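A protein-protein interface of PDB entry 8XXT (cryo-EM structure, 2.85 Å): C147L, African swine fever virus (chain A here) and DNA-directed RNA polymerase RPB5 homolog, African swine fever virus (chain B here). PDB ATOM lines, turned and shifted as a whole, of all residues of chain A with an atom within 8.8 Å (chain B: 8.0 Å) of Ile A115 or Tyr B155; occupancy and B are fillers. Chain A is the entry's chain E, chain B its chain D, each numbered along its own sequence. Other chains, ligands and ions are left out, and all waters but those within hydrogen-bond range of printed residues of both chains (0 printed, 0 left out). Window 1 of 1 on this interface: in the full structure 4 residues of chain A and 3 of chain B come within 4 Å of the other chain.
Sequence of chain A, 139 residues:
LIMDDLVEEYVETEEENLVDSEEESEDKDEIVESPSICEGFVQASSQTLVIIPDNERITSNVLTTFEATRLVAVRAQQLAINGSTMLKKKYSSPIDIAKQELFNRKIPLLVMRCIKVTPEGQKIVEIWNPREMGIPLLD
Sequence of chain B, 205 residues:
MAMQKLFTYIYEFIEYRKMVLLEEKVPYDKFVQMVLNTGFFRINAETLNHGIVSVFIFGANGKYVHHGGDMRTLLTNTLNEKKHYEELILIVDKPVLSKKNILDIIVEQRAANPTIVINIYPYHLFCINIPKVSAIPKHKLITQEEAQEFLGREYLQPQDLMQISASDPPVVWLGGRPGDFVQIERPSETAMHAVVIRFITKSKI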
ATOM      1  N   VAL A  50       3.475 -22.222  -4.067  1.00  0.00           N
ATOM      2  CA  VAL A  50       2.333 -23.124  -4.073  1.00  0.00           C
ATOM      3  C   VAL A  50       1.116 -22.337  -3.618  1.00  0.00           C
ATOM      4  O   VAL A  50       1.043 -21.900  -2.466  1.00  0.00           O
ATOM      5  CB  VAL A  50       2.570 -24.344  -3.172  1.00  0.00           C
ATOM      6  CG1 VAL A  50       1.272 -25.090  -2.958  1.00  0.00           C
ATOM      7  CG2 VAL A  50       3.595 -25.253  -3.801  1.00  0.00           C
ATOM      8  N   ILE A  51       0.163 -22.154  -4.522  1.00  0.00           N
ATOM      9  CA  ILE A  51      -1.058 -21.419  -4.223  1.00  0.00           C
ATOM     10  C   ILE A  51      -2.110 -22.419  -3.772  1.00  0.00           C
ATOM     11  O   ILE A  51      -2.498 -23.310  -4.534  1.00  0.00           O
ATOM     12  CB  ILE A  51      -1.536 -20.617  -5.441  1.00  0.00           C
ATOM     13  CG1 ILE A  51      -0.607 -19.430  -5.684  1.00  0.00           C
ATOM     14  CG2 ILE A  51      -2.957 -20.139  -5.240  1.00  0.00           C
ATOM     15  CD1 ILE A  51      -0.650 -18.905  -7.091  1.00  0.00           C
ATOM     16  N   ILE A  52      -2.562 -22.278  -2.531  1.00  0.00           N
ATOM     17  CA  ILE A  52      -3.555 -23.210  -1.990  1.00  0.00           C
ATOM     18  C   ILE A  52      -4.856 -23.058  -2.765  1.00  0.00           C
ATOM     19  O   ILE A  52      -5.298 -21.919  -3.013  1.00  0.00           O
ATOM     20  CB  ILE A  52      -3.769 -22.953  -0.490  1.00  0.00           C
ATOM     21  CG1 ILE A  52      -2.618 -23.550   0.314  1.00  0.00           C
ATOM     22  CG2 ILE A  52      -5.082 -23.536  -0.023  1.00  0.00           C
ATOM     23  CD1 ILE A  52      -2.613 -23.138   1.761  1.00  0.00           C
ATOM     24  N   PRO A  53      -5.500 -24.149  -3.179  1.00  0.00           N
ATOM     25  CA  PRO A  53      -6.715 -24.029  -3.990  1.00  0.00           C
ATOM     26  C   PRO A  53      -7.820 -23.301  -3.243  1.00  0.00           C
ATOM     27  O   PRO A  53      -7.896 -23.331  -2.014  1.00  0.00           O
ATOM     28  CB  PRO A  53      -7.095 -25.486  -4.274  1.00  0.00           C
ATOM     29  CG  PRO A  53      -5.817 -26.234  -4.137  1.00  0.00           C
ATOM     30  CD  PRO A  53      -5.071 -25.548  -3.038  1.00  0.00           C
ATOM     31  N   GLU A  56      -9.557 -24.969  -0.450  1.00  0.00           N
ATOM     32  CA  GLU A  56      -8.768 -25.438   0.680  1.00  0.00           C
ATOM     33  C   GLU A  56      -8.260 -24.305   1.557  1.00  0.00           C
ATOM     34  O   GLU A  56      -7.470 -24.557   2.471  1.00  0.00           O
ATOM     35  CB  GLU A  56      -7.585 -26.275   0.190  1.00  0.00           C
ATOM     36  CG  GLU A  56      -7.958 -27.379  -0.778  1.00  0.00           C
ATOM     37  CD  GLU A  56      -6.934 -28.492  -0.804  1.00  0.00           C
ATOM     38  OE1 GLU A  56      -5.730 -28.195  -0.672  1.00  0.00           O
ATOM     39  OE2 GLU A  56      -7.333 -29.666  -0.952  1.00  0.00           O
ATOM     40  N   ARG A  57      -8.685 -23.072   1.305  1.00  0.00           N
ATOM     41  CA  ARG A  57      -8.222 -21.936   2.084  1.00  0.00           C
ATOM     42  C   ARG A  57      -8.964 -21.879   3.410  1.00  0.00           C
ATOM     43  O   ARG A  57     -10.198 -21.916   3.442  1.00  0.00           O
ATOM     44  CB  ARG A  57      -8.423 -20.642   1.301  1.00  0.00           C
ATOM     45  CG  ARG A  57      -7.452 -20.476   0.152  1.00  0.00           C
ATOM     46  CD  ARG A  57      -7.766 -19.246  -0.659  1.00  0.00           C
ATOM     47  NE  ARG A  57      -9.182 -19.154  -0.979  1.00  0.00           N
ATOM     48  CZ  ARG A  57      -9.708 -18.220  -1.756  1.00  0.00           C
ATOM     49  NH1 ARG A  57      -8.962 -17.279  -2.307  1.00  0.00           N
ATOM     50  NH2 ARG A  57     -11.016 -18.230  -1.986  1.00  0.00           N
ATOM     51  N   ILE A  58      -8.212 -21.783   4.504  1.00  0.00           N
ATOM     52  CA  ILE A  58      -8.776 -21.779   5.846  1.00  0.00           C
ATOM     53  C   ILE A  58      -8.566 -20.460   6.565  1.00  0.00           C
ATOM     54  O   ILE A  58      -8.831 -20.377   7.767  1.00  0.00           O
ATOM     55  CB  ILE A  58      -8.216 -22.939   6.694  1.00  0.00           C
ATOM     56  CG1 ILE A  58      -6.724 -22.743   6.939  1.00  0.00           C
ATOM     57  CG2 ILE A  58      -8.482 -24.267   6.015  1.00  0.00           C
ATOM     58  CD1 ILE A  58      -6.048 -23.950   7.519  1.00  0.00           C
ATOM     59  N   THR A  59      -8.091 -19.432   5.879  1.00  0.00           N
ATOM     60  CA  THR A  59      -7.950 -18.125   6.493  1.00  0.00           C
ATOM     61  C   THR A  59      -9.230 -17.321   6.304  1.00  0.00           C
ATOM     62  O   THR A  59     -10.090 -17.655   5.490  1.00  0.00           O
ATOM     63  CB  THR A  59      -6.752 -17.386   5.906  1.00  0.00           C
ATOM     64  OG1 THR A  59      -6.700 -17.612   4.492  1.00  0.00           O
ATOM     65  CG2 THR A  59      -5.472 -17.894   6.532  1.00  0.00           C
ATOM     66  N   SER A  60      -9.351 -16.246   7.078  1.00  0.00           N
ATOM     67  CA  SER A  60     -10.573 -15.455   7.079  1.00  0.00           C
ATOM     68  C   SER A  60     -10.852 -14.874   5.702  1.00  0.00           C
ATOM     69  O   SER A  60      -9.955 -14.366   5.027  1.00  0.00           O
ATOM     70  CB  SER A  60     -10.471 -14.327   8.102  1.00  0.00           C
ATOM     71  OG  SER A  60     -11.411 -13.306   7.826  1.00  0.00           O
ATOM     72  N   MET A 112      -1.966 -11.795  -0.885  1.00  0.00           N
ATOM     73  CA  MET A 112      -1.301 -13.081  -0.750  1.00  0.00           C
ATOM     74  C   MET A 112      -0.947 -13.275   0.716  1.00  0.00           C
ATOM     75  O   MET A 112      -0.184 -12.489   1.284  1.00  0.00           O
ATOM     76  CB  MET A 112      -0.055 -13.154  -1.629  1.00  0.00           C
ATOM     77  CG  MET A 112       1.038 -14.053  -1.089  1.00  0.00           C
ATOM     78  SD  MET A 112       2.398 -14.270  -2.243  1.00  0.00           S
ATOM     79  CE  MET A 112       1.503 -14.688  -3.731  1.00  0.00           C
ATOM     80  N   ARG A 113      -1.523 -14.301   1.328  1.00  0.00           N
ATOM     81  CA  ARG A 113      -1.248 -14.657   2.711  1.00  0.00           C
ATOM     82  C   ARG A 113      -0.358 -15.886   2.706  1.00  0.00           C
ATOM     83  O   ARG A 113      -0.761 -16.941   2.210  1.00  0.00           O
ATOM     84  CB  ARG A 113      -2.541 -14.931   3.475  1.00  0.00           C
ATOM     85  CG  ARG A 113      -3.490 -13.758   3.510  1.00  0.00           C
ATOM     86  CD  ARG A 113      -4.776 -14.119   4.213  1.00  0.00           C
ATOM     87  NE  ARG A 113      -5.529 -12.931   4.587  1.00  0.00           N
ATOM     88  CZ  ARG A 113      -6.823 -12.924   4.868  1.00  0.00           C
ATOM     89  NH1 ARG A 113      -7.544 -14.029   4.822  1.00  0.00           N
ATOM     90  NH2 ARG A 113      -7.404 -11.780   5.209  1.00  0.00           N
ATOM     91  N   CYS A 114       0.842 -15.751   3.249  1.00  0.00           N
ATOM     92  CA  CYS A 114       1.836 -16.815   3.215  1.00  0.00           C
ATOM     93  C   CYS A 114       1.770 -17.601   4.515  1.00  0.00           C
ATOM     94  O   CYS A 114       2.086 -17.068   5.582  1.00  0.00           O
ATOM     95  CB  CYS A 114       3.234 -16.239   3.002  1.00  0.00           C
ATOM     96  SG  CYS A 114       4.570 -17.429   3.247  1.00  0.00           S
ATOM     97  N   ILE A 115       1.362 -18.866   4.435  1.00  0.00           N
ATOM     98  CA  ILE A 115       1.540 -19.738   5.587  1.00  0.00           C
ATOM     99  C   ILE A 115       2.277 -21.012   5.208  1.00  0.00           C
ATOM    100  O   ILE A 115       1.685 -22.095   5.143  1.00  0.00           O
ATOM    101  CB  ILE A 115       0.175 -20.062   6.223  1.00  0.00           C
ATOM    102  CG1 ILE A 115      -0.792 -20.660   5.195  1.00  0.00           C
ATOM    103  CG2 ILE A 115      -0.422 -18.843   6.845  1.00  0.00           C
ATOM    104  CD1 ILE A 115      -2.212 -20.748   5.684  1.00  0.00           C
ATOM    105  N   LYS A 116       3.589 -20.887   5.001  1.00  0.00           N
ATOM    106  CA  LYS A 116       4.591 -21.924   5.207  1.00  0.00           C
ATOM    107  C   LYS A 116       5.916 -21.428   4.652  1.00  0.00           C
ATOM    108  O   LYS A 116       5.941 -20.534   3.803  1.00  0.00           O
ATOM    109  CB  LYS A 116       4.214 -23.255   4.560  1.00  0.00           C
ATOM    110  CG  LYS A 116       4.845 -24.446   5.249  1.00  0.00           C
ATOM    111  CD  LYS A 116       4.791 -24.293   6.756  1.00  0.00           C
ATOM    112  CE  LYS A 116       5.701 -25.296   7.440  1.00  0.00           C
ATOM    113  NZ  LYS A 116       5.394 -26.696   7.042  1.00  0.00           N
ATOM    114  N   VAL A 117       7.019 -22.006   5.113  1.00  0.00           N
ATOM    115  CA  VAL A 117       8.270 -22.007   4.369  1.00  0.00           C
ATOM    116  C   VAL A 117       8.810 -23.428   4.459  1.00  0.00           C
ATOM    117  O   VAL A 117       9.515 -23.771   5.413  1.00  0.00           O
ATOM    118  CB  VAL A 117       9.286 -20.984   4.895  1.00  0.00           C
ATOM    119  CG1 VAL A 117       8.980 -19.616   4.318  1.00  0.00           C
ATOM    120  CG2 VAL A 117       9.244 -20.915   6.414  1.00  0.00           C
ATOM    121  N   THR A 118       8.476 -24.249   3.478  1.00  0.00           N
ATOM    122  CA  THR A 118       8.880 -25.645   3.518  1.00  0.00           C
ATOM    123  C   THR A 118      10.379 -25.761   3.256  1.00  0.00           C
ATOM    124  O   THR A 118      10.911 -25.052   2.398  1.00  0.00           O
ATOM    125  CB  THR A 118       8.106 -26.447   2.480  1.00  0.00           C
ATOM    126  OG1 THR A 118       6.725 -26.072   2.532  1.00  0.00           O
ATOM    127  CG2 THR A 118       8.213 -27.932   2.750  1.00  0.00           C
ATOM    128  N   GLN A 122       9.737 -24.325  -0.696  1.00  0.00           N
ATOM    129  CA  GLN A 122       8.350 -24.289  -1.136  1.00  0.00           C
ATOM    130  C   GLN A 122       7.609 -23.261  -0.302  1.00  0.00           C
ATOM    131  O   GLN A 122       7.530 -23.398   0.920  1.00  0.00           O
ATOM    132  CB  GLN A 122       7.707 -25.668  -0.992  1.00  0.00           C
ATOM    133  CG  GLN A 122       6.315 -25.775  -1.546  1.00  0.00           C
ATOM    134  CD  GLN A 122       6.148 -27.002  -2.412  1.00  0.00           C
ATOM    135  OE1 GLN A 122       6.668 -27.062  -3.525  1.00  0.00           O
ATOM    136  NE2 GLN A 122       5.425 -27.992  -1.905  1.00  0.00           N
ATOM    137  N   LYS A 123       7.075 -22.236  -0.952  1.00  0.00           N
ATOM    138  CA  LYS A 123       6.348 -21.172  -0.273  1.00  0.00           C
ATOM    139  C   LYS A 123       4.862 -21.387  -0.515  1.00  0.00           C
ATOM    140  O   LYS A 123       4.373 -21.176  -1.629  1.00  0.00           O
ATOM    141  CB  LYS A 123       6.792 -19.799  -0.766  1.00  0.00           C
ATOM    142  CG  LYS A 123       6.303 -18.652   0.089  1.00  0.00           C
ATOM    143  CD  LYS A 123       6.784 -17.328  -0.462  1.00  0.00           C
ATOM    144  CE  LYS A 123       6.233 -16.167   0.333  1.00  0.00           C
ATOM    145  NZ  LYS A 123       6.500 -14.871  -0.339  1.00  0.00           N
ATOM    146  N   ILE A 124       4.146 -21.793   0.527  1.00  0.00           N
ATOM    147  CA  ILE A 124       2.723 -22.089   0.440  1.00  0.00           C
ATOM    148  C   ILE A 124       1.954 -20.840   0.840  1.00  0.00           C
ATOM    149  O   ILE A 124       2.143 -20.310   1.940  1.00  0.00           O
ATOM    150  CB  ILE A 124       2.347 -23.284   1.326  1.00  0.00           C
ATOM    151  CG1 ILE A 124       3.343 -24.422   1.108  1.00  0.00           C
ATOM    152  CG2 ILE A 124       0.947 -23.746   1.014  1.00  0.00           C
ATOM    153  CD1 ILE A 124       2.998 -25.687   1.840  1.00  0.00           C
ATOM    154  N   VAL A 125       1.087 -20.366  -0.052  1.00  0.00           N
ATOM    155  CA  VAL A 125       0.355 -19.126   0.150  1.00  0.00           C
ATOM    156  C   VAL A 125      -1.116 -19.347  -0.164  1.00  0.00           C
ATOM    157  O   VAL A 125      -1.501 -20.310  -0.828  1.00  0.00           O
ATOM    158  CB  VAL A 125       0.905 -17.978  -0.717  1.00  0.00           C
ATOM    159  CG1 VAL A 125       2.335 -17.662  -0.340  1.00  0.00           C
ATOM    160  CG2 VAL A 125       0.807 -18.338  -2.182  1.00  0.00           C
ATOM    161  N   GLU A 126      -1.942 -18.435   0.341  1.00  0.00           N
ATOM    162  CA  GLU A 126      -3.349 -18.339  -0.023  1.00  0.00           C
ATOM    163  C   GLU A 126      -3.572 -16.971  -0.639  1.00  0.00           C
ATOM    164  O   GLU A 126      -3.420 -15.952   0.041  1.00  0.00           O
ATOM    165  CB  GLU A 126      -4.256 -18.525   1.194  1.00  0.00           C
ATOM    166  CG  GLU A 126      -3.983 -19.776   1.999  1.00  0.00           C
ATOM    167  CD  GLU A 126      -5.043 -20.027   3.051  1.00  0.00           C
ATOM    168  OE1 GLU A 126      -6.007 -19.241   3.125  1.00  0.00           O
ATOM    169  OE2 GLU A 126      -4.913 -21.007   3.810  1.00  0.00           O
ATOM    170  N   ILE A 127      -3.928 -16.942  -1.917  1.00  0.00           N
ATOM    171  CA  ILE A 127      -4.191 -15.695  -2.621  1.00  0.00           C
ATOM    172  C   ILE A 127      -5.671 -15.382  -2.484  1.00  0.00           C
ATOM    173  O   ILE A 127      -6.524 -16.163  -2.922  1.00  0.00           O
ATOM    174  CB  ILE A 127      -3.773 -15.777  -4.096  1.00  0.00           C
ATOM    175  CG1 ILE A 127      -2.251 -15.741  -4.208  1.00  0.00           C
ATOM    176  CG2 ILE A 127      -4.389 -14.640  -4.882  1.00  0.00           C
ATOM    177  CD1 ILE A 127      -1.750 -15.671  -5.623  1.00  0.00           C
ATOM    178  N   TRP A 128      -5.976 -14.243  -1.877  1.00  0.00           N
ATOM    179  CA  TRP A 128      -7.340 -13.850  -1.566  1.00  0.00           C
ATOM    180  C   TRP A 128      -7.719 -12.644  -2.407  1.00  0.00           C
ATOM    181  O   TRP A 128      -6.933 -11.703  -2.539  1.00  0.00           O
ATOM    182  CB  TRP A 128      -7.477 -13.525  -0.081  1.00  0.00           C
ATOM    183  CG  TRP A 128      -7.771 -14.714   0.763  1.00  0.00           C
ATOM    184  CD1 TRP A 128      -6.880 -15.441   1.488  1.00  0.00           C
ATOM    185  CD2 TRP A 128      -9.050 -15.312   0.981  1.00  0.00           C
ATOM    186  NE1 TRP A 128      -7.522 -16.458   2.141  1.00  0.00           N
ATOM    187  CE2 TRP A 128      -8.857 -16.400   1.847  1.00  0.00           C
ATOM    188  CE3 TRP A 128     -10.339 -15.033   0.526  1.00  0.00           C
ATOM    189  CZ2 TRP A 128      -9.903 -17.211   2.267  1.00  0.00           C
ATOM    190  CZ3 TRP A 128     -11.372 -15.835   0.943  1.00  0.00           C
ATOM    191  CH2 TRP A 128     -11.151 -16.912   1.806  1.00  0.00           C
ATOM    192  N   GLN B 148      -0.588 -35.866  14.114  1.00  0.00           N
ATOM    193  CA  GLN B 148      -0.053 -35.555  12.794  1.00  0.00           C
ATOM    194  C   GLN B 148      -1.091 -34.870  11.918  1.00  0.00           C
ATOM    195  O   GLN B 148      -0.757 -33.955  11.162  1.00  0.00           O
ATOM    196  CB  GLN B 148       0.462 -36.823  12.119  1.00  0.00           C
ATOM    197  CG  GLN B 148       0.863 -36.625  10.667  1.00  0.00           C
ATOM    198  CD  GLN B 148       1.952 -35.586  10.501  1.00  0.00           C
ATOM    199  OE1 GLN B 148       2.911 -35.546  11.273  1.00  0.00           O
ATOM    200  NE2 GLN B 148       1.805 -34.729   9.497  1.00  0.00           N
ATOM    201  N   GLU B 149      -2.351 -35.300  11.988  1.00  0.00           N
ATOM    202  CA  GLU B 149      -3.380 -34.635  11.196  1.00  0.00           C
ATOM    203  C   GLU B 149      -3.643 -33.225  11.715  1.00  0.00           C
ATOM    204  O   GLU B 149      -3.870 -32.298  10.925  1.00  0.00           O
ATOM    205  CB  GLU B 149      -4.663 -35.468  11.171  1.00  0.00           C
ATOM    206  CG  GLU B 149      -5.487 -35.439  12.440  1.00  0.00           C
ATOM    207  CD  GLU B 149      -6.962 -35.662  12.189  1.00  0.00           C
ATOM    208  OE1 GLU B 149      -7.632 -34.726  11.704  1.00  0.00           O
ATOM    209  OE2 GLU B 149      -7.452 -36.775  12.479  1.00  0.00           O
ATOM    210  N   PHE B 150      -3.588 -33.037  13.038  1.00  0.00           N
ATOM    211  CA  PHE B 150      -3.692 -31.691  13.589  1.00  0.00           C
ATOM    212  C   PHE B 150      -2.559 -30.808  13.089  1.00  0.00           C
ATOM    213  O   PHE B 150      -2.779 -29.649  12.724  1.00  0.00           O
ATOM    214  CB  PHE B 150      -3.693 -31.749  15.117  1.00  0.00           C
ATOM    215  CG  PHE B 150      -3.221 -30.485  15.772  1.00  0.00           C
ATOM    216  CD1 PHE B 150      -4.045 -29.379  15.844  1.00  0.00           C
ATOM    217  CD2 PHE B 150      -1.954 -30.403  16.316  1.00  0.00           C
ATOM    218  CE1 PHE B 150      -3.613 -28.218  16.445  1.00  0.00           C
ATOM    219  CE2 PHE B 150      -1.519 -29.242  16.916  1.00  0.00           C
ATOM    220  CZ  PHE B 150      -2.349 -28.150  16.981  1.00  0.00           C
ATOM    221  N   LEU B 151      -1.337 -31.342  13.067  1.00  0.00           N
ATOM    222  CA  LEU B 151      -0.199 -30.578  12.568  1.00  0.00           C
ATOM    223  C   LEU B 151      -0.350 -30.269  11.085  1.00  0.00           C
ATOM    224  O   LEU B 151      -0.036 -29.161  10.638  1.00  0.00           O
ATOM    225  CB  LEU B 151       1.097 -31.342  12.822  1.00  0.00           C
ATOM    226  CG  LEU B 151       1.534 -31.483  14.277  1.00  0.00           C
ATOM    227  CD1 LEU B 151       2.777 -32.342  14.366  1.00  0.00           C
ATOM    228  CD2 LEU B 151       1.775 -30.121  14.889  1.00  0.00           C
ATOM    229  N   GLY B 152      -0.826 -31.239  10.307  1.00  0.00           N
ATOM    230  CA  GLY B 152      -0.983 -31.026   8.879  1.00  0.00           C
ATOM    231  C   GLY B 152      -2.006 -29.955   8.560  1.00  0.00           C
ATOM    232  O   GLY B 152      -1.815 -29.157   7.641  1.00  0.00           O
ATOM    233  N   ARG B 153      -3.111 -29.929   9.307  1.00  0.00           N
ATOM    234  CA  ARG B 153      -4.064 -28.837   9.142  1.00  0.00           C
ATOM    235  C   ARG B 153      -3.442 -27.506   9.534  1.00  0.00           C
ATOM    236  O   ARG B 153      -3.684 -26.482   8.885  1.00  0.00           O
ATOM    237  CB  ARG B 153      -5.321 -29.100   9.966  1.00  0.00           C
ATOM    238  CG  ARG B 153      -6.462 -28.154   9.652  1.00  0.00           C
ATOM    239  CD  ARG B 153      -6.746 -27.218  10.807  1.00  0.00           C
ATOM    240  NE  ARG B 153      -7.726 -26.204  10.444  1.00  0.00           N
ATOM    241  CZ  ARG B 153      -7.773 -24.989  10.971  1.00  0.00           C
ATOM    242  NH1 ARG B 153      -6.922 -24.610  11.908  1.00  0.00           N
ATOM    243  NH2 ARG B 153      -8.695 -24.132  10.544  1.00  0.00           N
ATOM    244  N   GLU B 154      -2.634 -27.500  10.592  1.00  0.00           N
ATOM    245  CA  GLU B 154      -2.032 -26.278  11.103  1.00  0.00           C
ATOM    246  C   GLU B 154      -0.734 -25.904  10.405  1.00  0.00           C
ATOM    247  O   GLU B 154      -0.218 -24.810  10.651  1.00  0.00           O
ATOM    248  CB  GLU B 154      -1.774 -26.414  12.605  1.00  0.00           C
ATOM    249  CG  GLU B 154      -3.030 -26.503  13.452  1.00  0.00           C
ATOM    250  CD  GLU B 154      -3.640 -25.149  13.735  1.00  0.00           C
ATOM    251  OE1 GLU B 154      -2.880 -24.211  14.054  1.00  0.00           O
ATOM    252  OE2 GLU B 154      -4.878 -25.020  13.646  1.00  0.00           O
ATOM    253  N   TYR B 155      -0.195 -26.774   9.552  1.00  0.00           N
ATOM    254  CA  TYR B 155       1.080 -26.546   8.875  1.00  0.00           C
ATOM    255  C   TYR B 155       2.188 -26.255   9.885  1.00  0.00           C
ATOM    256  O   TYR B 155       2.851 -25.218   9.849  1.00  0.00           O
ATOM    257  CB  TYR B 155       0.965 -25.418   7.847  1.00  0.00           C
ATOM    258  CG  TYR B 155       0.376 -25.844   6.527  1.00  0.00           C
ATOM    259  CD1 TYR B 155       0.661 -27.089   5.991  1.00  0.00           C
ATOM    260  CD2 TYR B 155      -0.462 -25.003   5.816  1.00  0.00           C
ATOM    261  CE1 TYR B 155       0.125 -27.485   4.784  1.00  0.00           C
ATOM    262  CE2 TYR B 155      -1.001 -25.389   4.609  1.00  0.00           C
ATOM    263  CZ  TYR B 155      -0.706 -26.630   4.098  1.00  0.00           C
ATOM    264  OH  TYR B 155      -1.242 -27.021   2.896  1.00  0.00           O
ATOM    265  N   LEU B 156       2.380 -27.199  10.801  1.00  0.00           N
ATOM    266  CA  LEU B 156       3.349 -27.059  11.873  1.00  0.00           C
ATOM    267  C   LEU B 156       4.224 -28.296  11.957  1.00  0.00           C
ATOM    268  O   LEU B 156       3.774 -29.416  11.703  1.00  0.00           O
ATOM    269  CB  LEU B 156       2.671 -26.847  13.227  1.00  0.00           C
ATOM    270  CG  LEU B 156       1.911 -25.547  13.455  1.00  0.00           C
ATOM    271  CD1 LEU B 156       1.170 -25.625  14.769  1.00  0.00           C
ATOM    272  CD2 LEU B 156       2.863 -24.370  13.446  1.00  0.00           C
ATOM    273  N   GLN B 157       5.480 -28.082  12.310  1.00  0.00           N
ATOM    274  CA  GLN B 157       6.346 -29.172  12.708  1.00  0.00           C
ATOM    275  C   GLN B 157       6.119 -29.483  14.182  1.00  0.00           C
ATOM    276  O   GLN B 157       5.651 -28.630  14.937  1.00  0.00           O
ATOM    277  CB  GLN B 157       7.806 -28.809  12.465  1.00  0.00           C
ATOM    278  CG  GLN B 157       8.271 -29.030  11.042  1.00  0.00           C
ATOM    279  CD  GLN B 157       7.730 -27.987  10.093  1.00  0.00           C
ATOM    280  OE1 GLN B 157       6.926 -28.288   9.212  1.00  0.00           O
ATOM    281  NE2 GLN B 157       8.166 -26.745  10.271  1.00  0.00           N
ATOM    282  N   PRO B 158       6.434 -30.703  14.617  1.00  0.00           N
ATOM    283  CA  PRO B 158       6.261 -31.028  16.039  1.00  0.00           C
ATOM    284  C   PRO B 158       7.054 -30.128  16.966  1.00  0.00           C
ATOM    285  O   PRO B 158       6.653 -29.934  18.119  1.00  0.00           O
ATOM    286  CB  PRO B 158       6.736 -32.483  16.119  1.00  0.00           C
ATOM    287  CG  PRO B 158       6.511 -33.020  14.759  1.00  0.00           C
ATOM    288  CD  PRO B 158       6.790 -31.888  13.821  1.00  0.00           C
ATOM    289  N   ASP B 160       7.477 -26.922  16.636  1.00  0.00           N
ATOM    290  CA  ASP B 160       6.913 -25.581  16.707  1.00  0.00           C
ATOM    291  C   ASP B 160       5.918 -25.418  17.845  1.00  0.00           C
ATOM    292  O   ASP B 160       5.574 -24.281  18.182  1.00  0.00           O
ATOM    293  CB  ASP B 160       6.232 -25.219  15.386  1.00  0.00           C
ATOM    294  CG  ASP B 160       7.218 -24.808  14.312  1.00  0.00           C
ATOM    295  OD1 ASP B 160       8.349 -24.413  14.660  1.00  0.00           O
ATOM    296  OD2 ASP B 160       6.860 -24.872  13.120  1.00  0.00           O
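Ile A52 touches Tyr B155 (CD1 to CE2, 3.97 Å). O of Arg B153 touches CD1 of Ile A58 (3.7 Å). O of Ile A115 touches CD2 of Tyr B155, at 3.7 Å. Tyr B155 touches Lys A116 (O to CE, 3.7 Å).
Of the 12 printed residues of chain B, 3 touch a printed residue of chain A. Hydrophobic or aromatic side chains of chain B within 4 Å of the printed part of chain A: Tyr B155.
NZ of Lys A116 is in hydrogen-bond range of OE1 of Gln B157 (3.1 Å).
Of chain B, only Tyr B155 comes within 4 Å of Ile A115. No residue of chain B comes within 4 Å of Cys A114. No residue of chain A comes within 4 Å of Gly B152. Of the printed residues of chain B, Ile A58 touches Arg B153 (3.7 Å). Printed residues of chain B within 4 Å of Lys A116: Tyr B155 (3.7 Å) and Gln B157 (3.1 Å). Printed residues of chain B within 4 Å of Ile A52: Tyr B155. Lys A123 touches none of the printed residues of chain B. Glu B154 touches none of the printed residues of chain A. The nearest printed residue of chain B that does not touch Lys A116 is Leu B156 (4.8 Å).
NH1 of Arg B153 is in salt-bridge range of OE2 of Glu B154 (2.7 Å). O of Val A125 sits at hydrogen-bond distance from N of Ile A52, at 2.8 Å. The side-chain carboxylate of Glu A126 sits at hydrogen-bond distance from the backbone NH of Ile A58 (3.5 Å). SG of Cys A114 is in hydrogen-bond range of O of Lys A116 (3.4 Å). N of Ile A115 sits at hydrogen-bond distance from O of Ile A124, at 3.0 Å. The backbone carbonyl oxygen (O) of Ile A124 lies within hydrogen-bond range of the backbone NH (N) of Lys A116 (3.4 Å).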
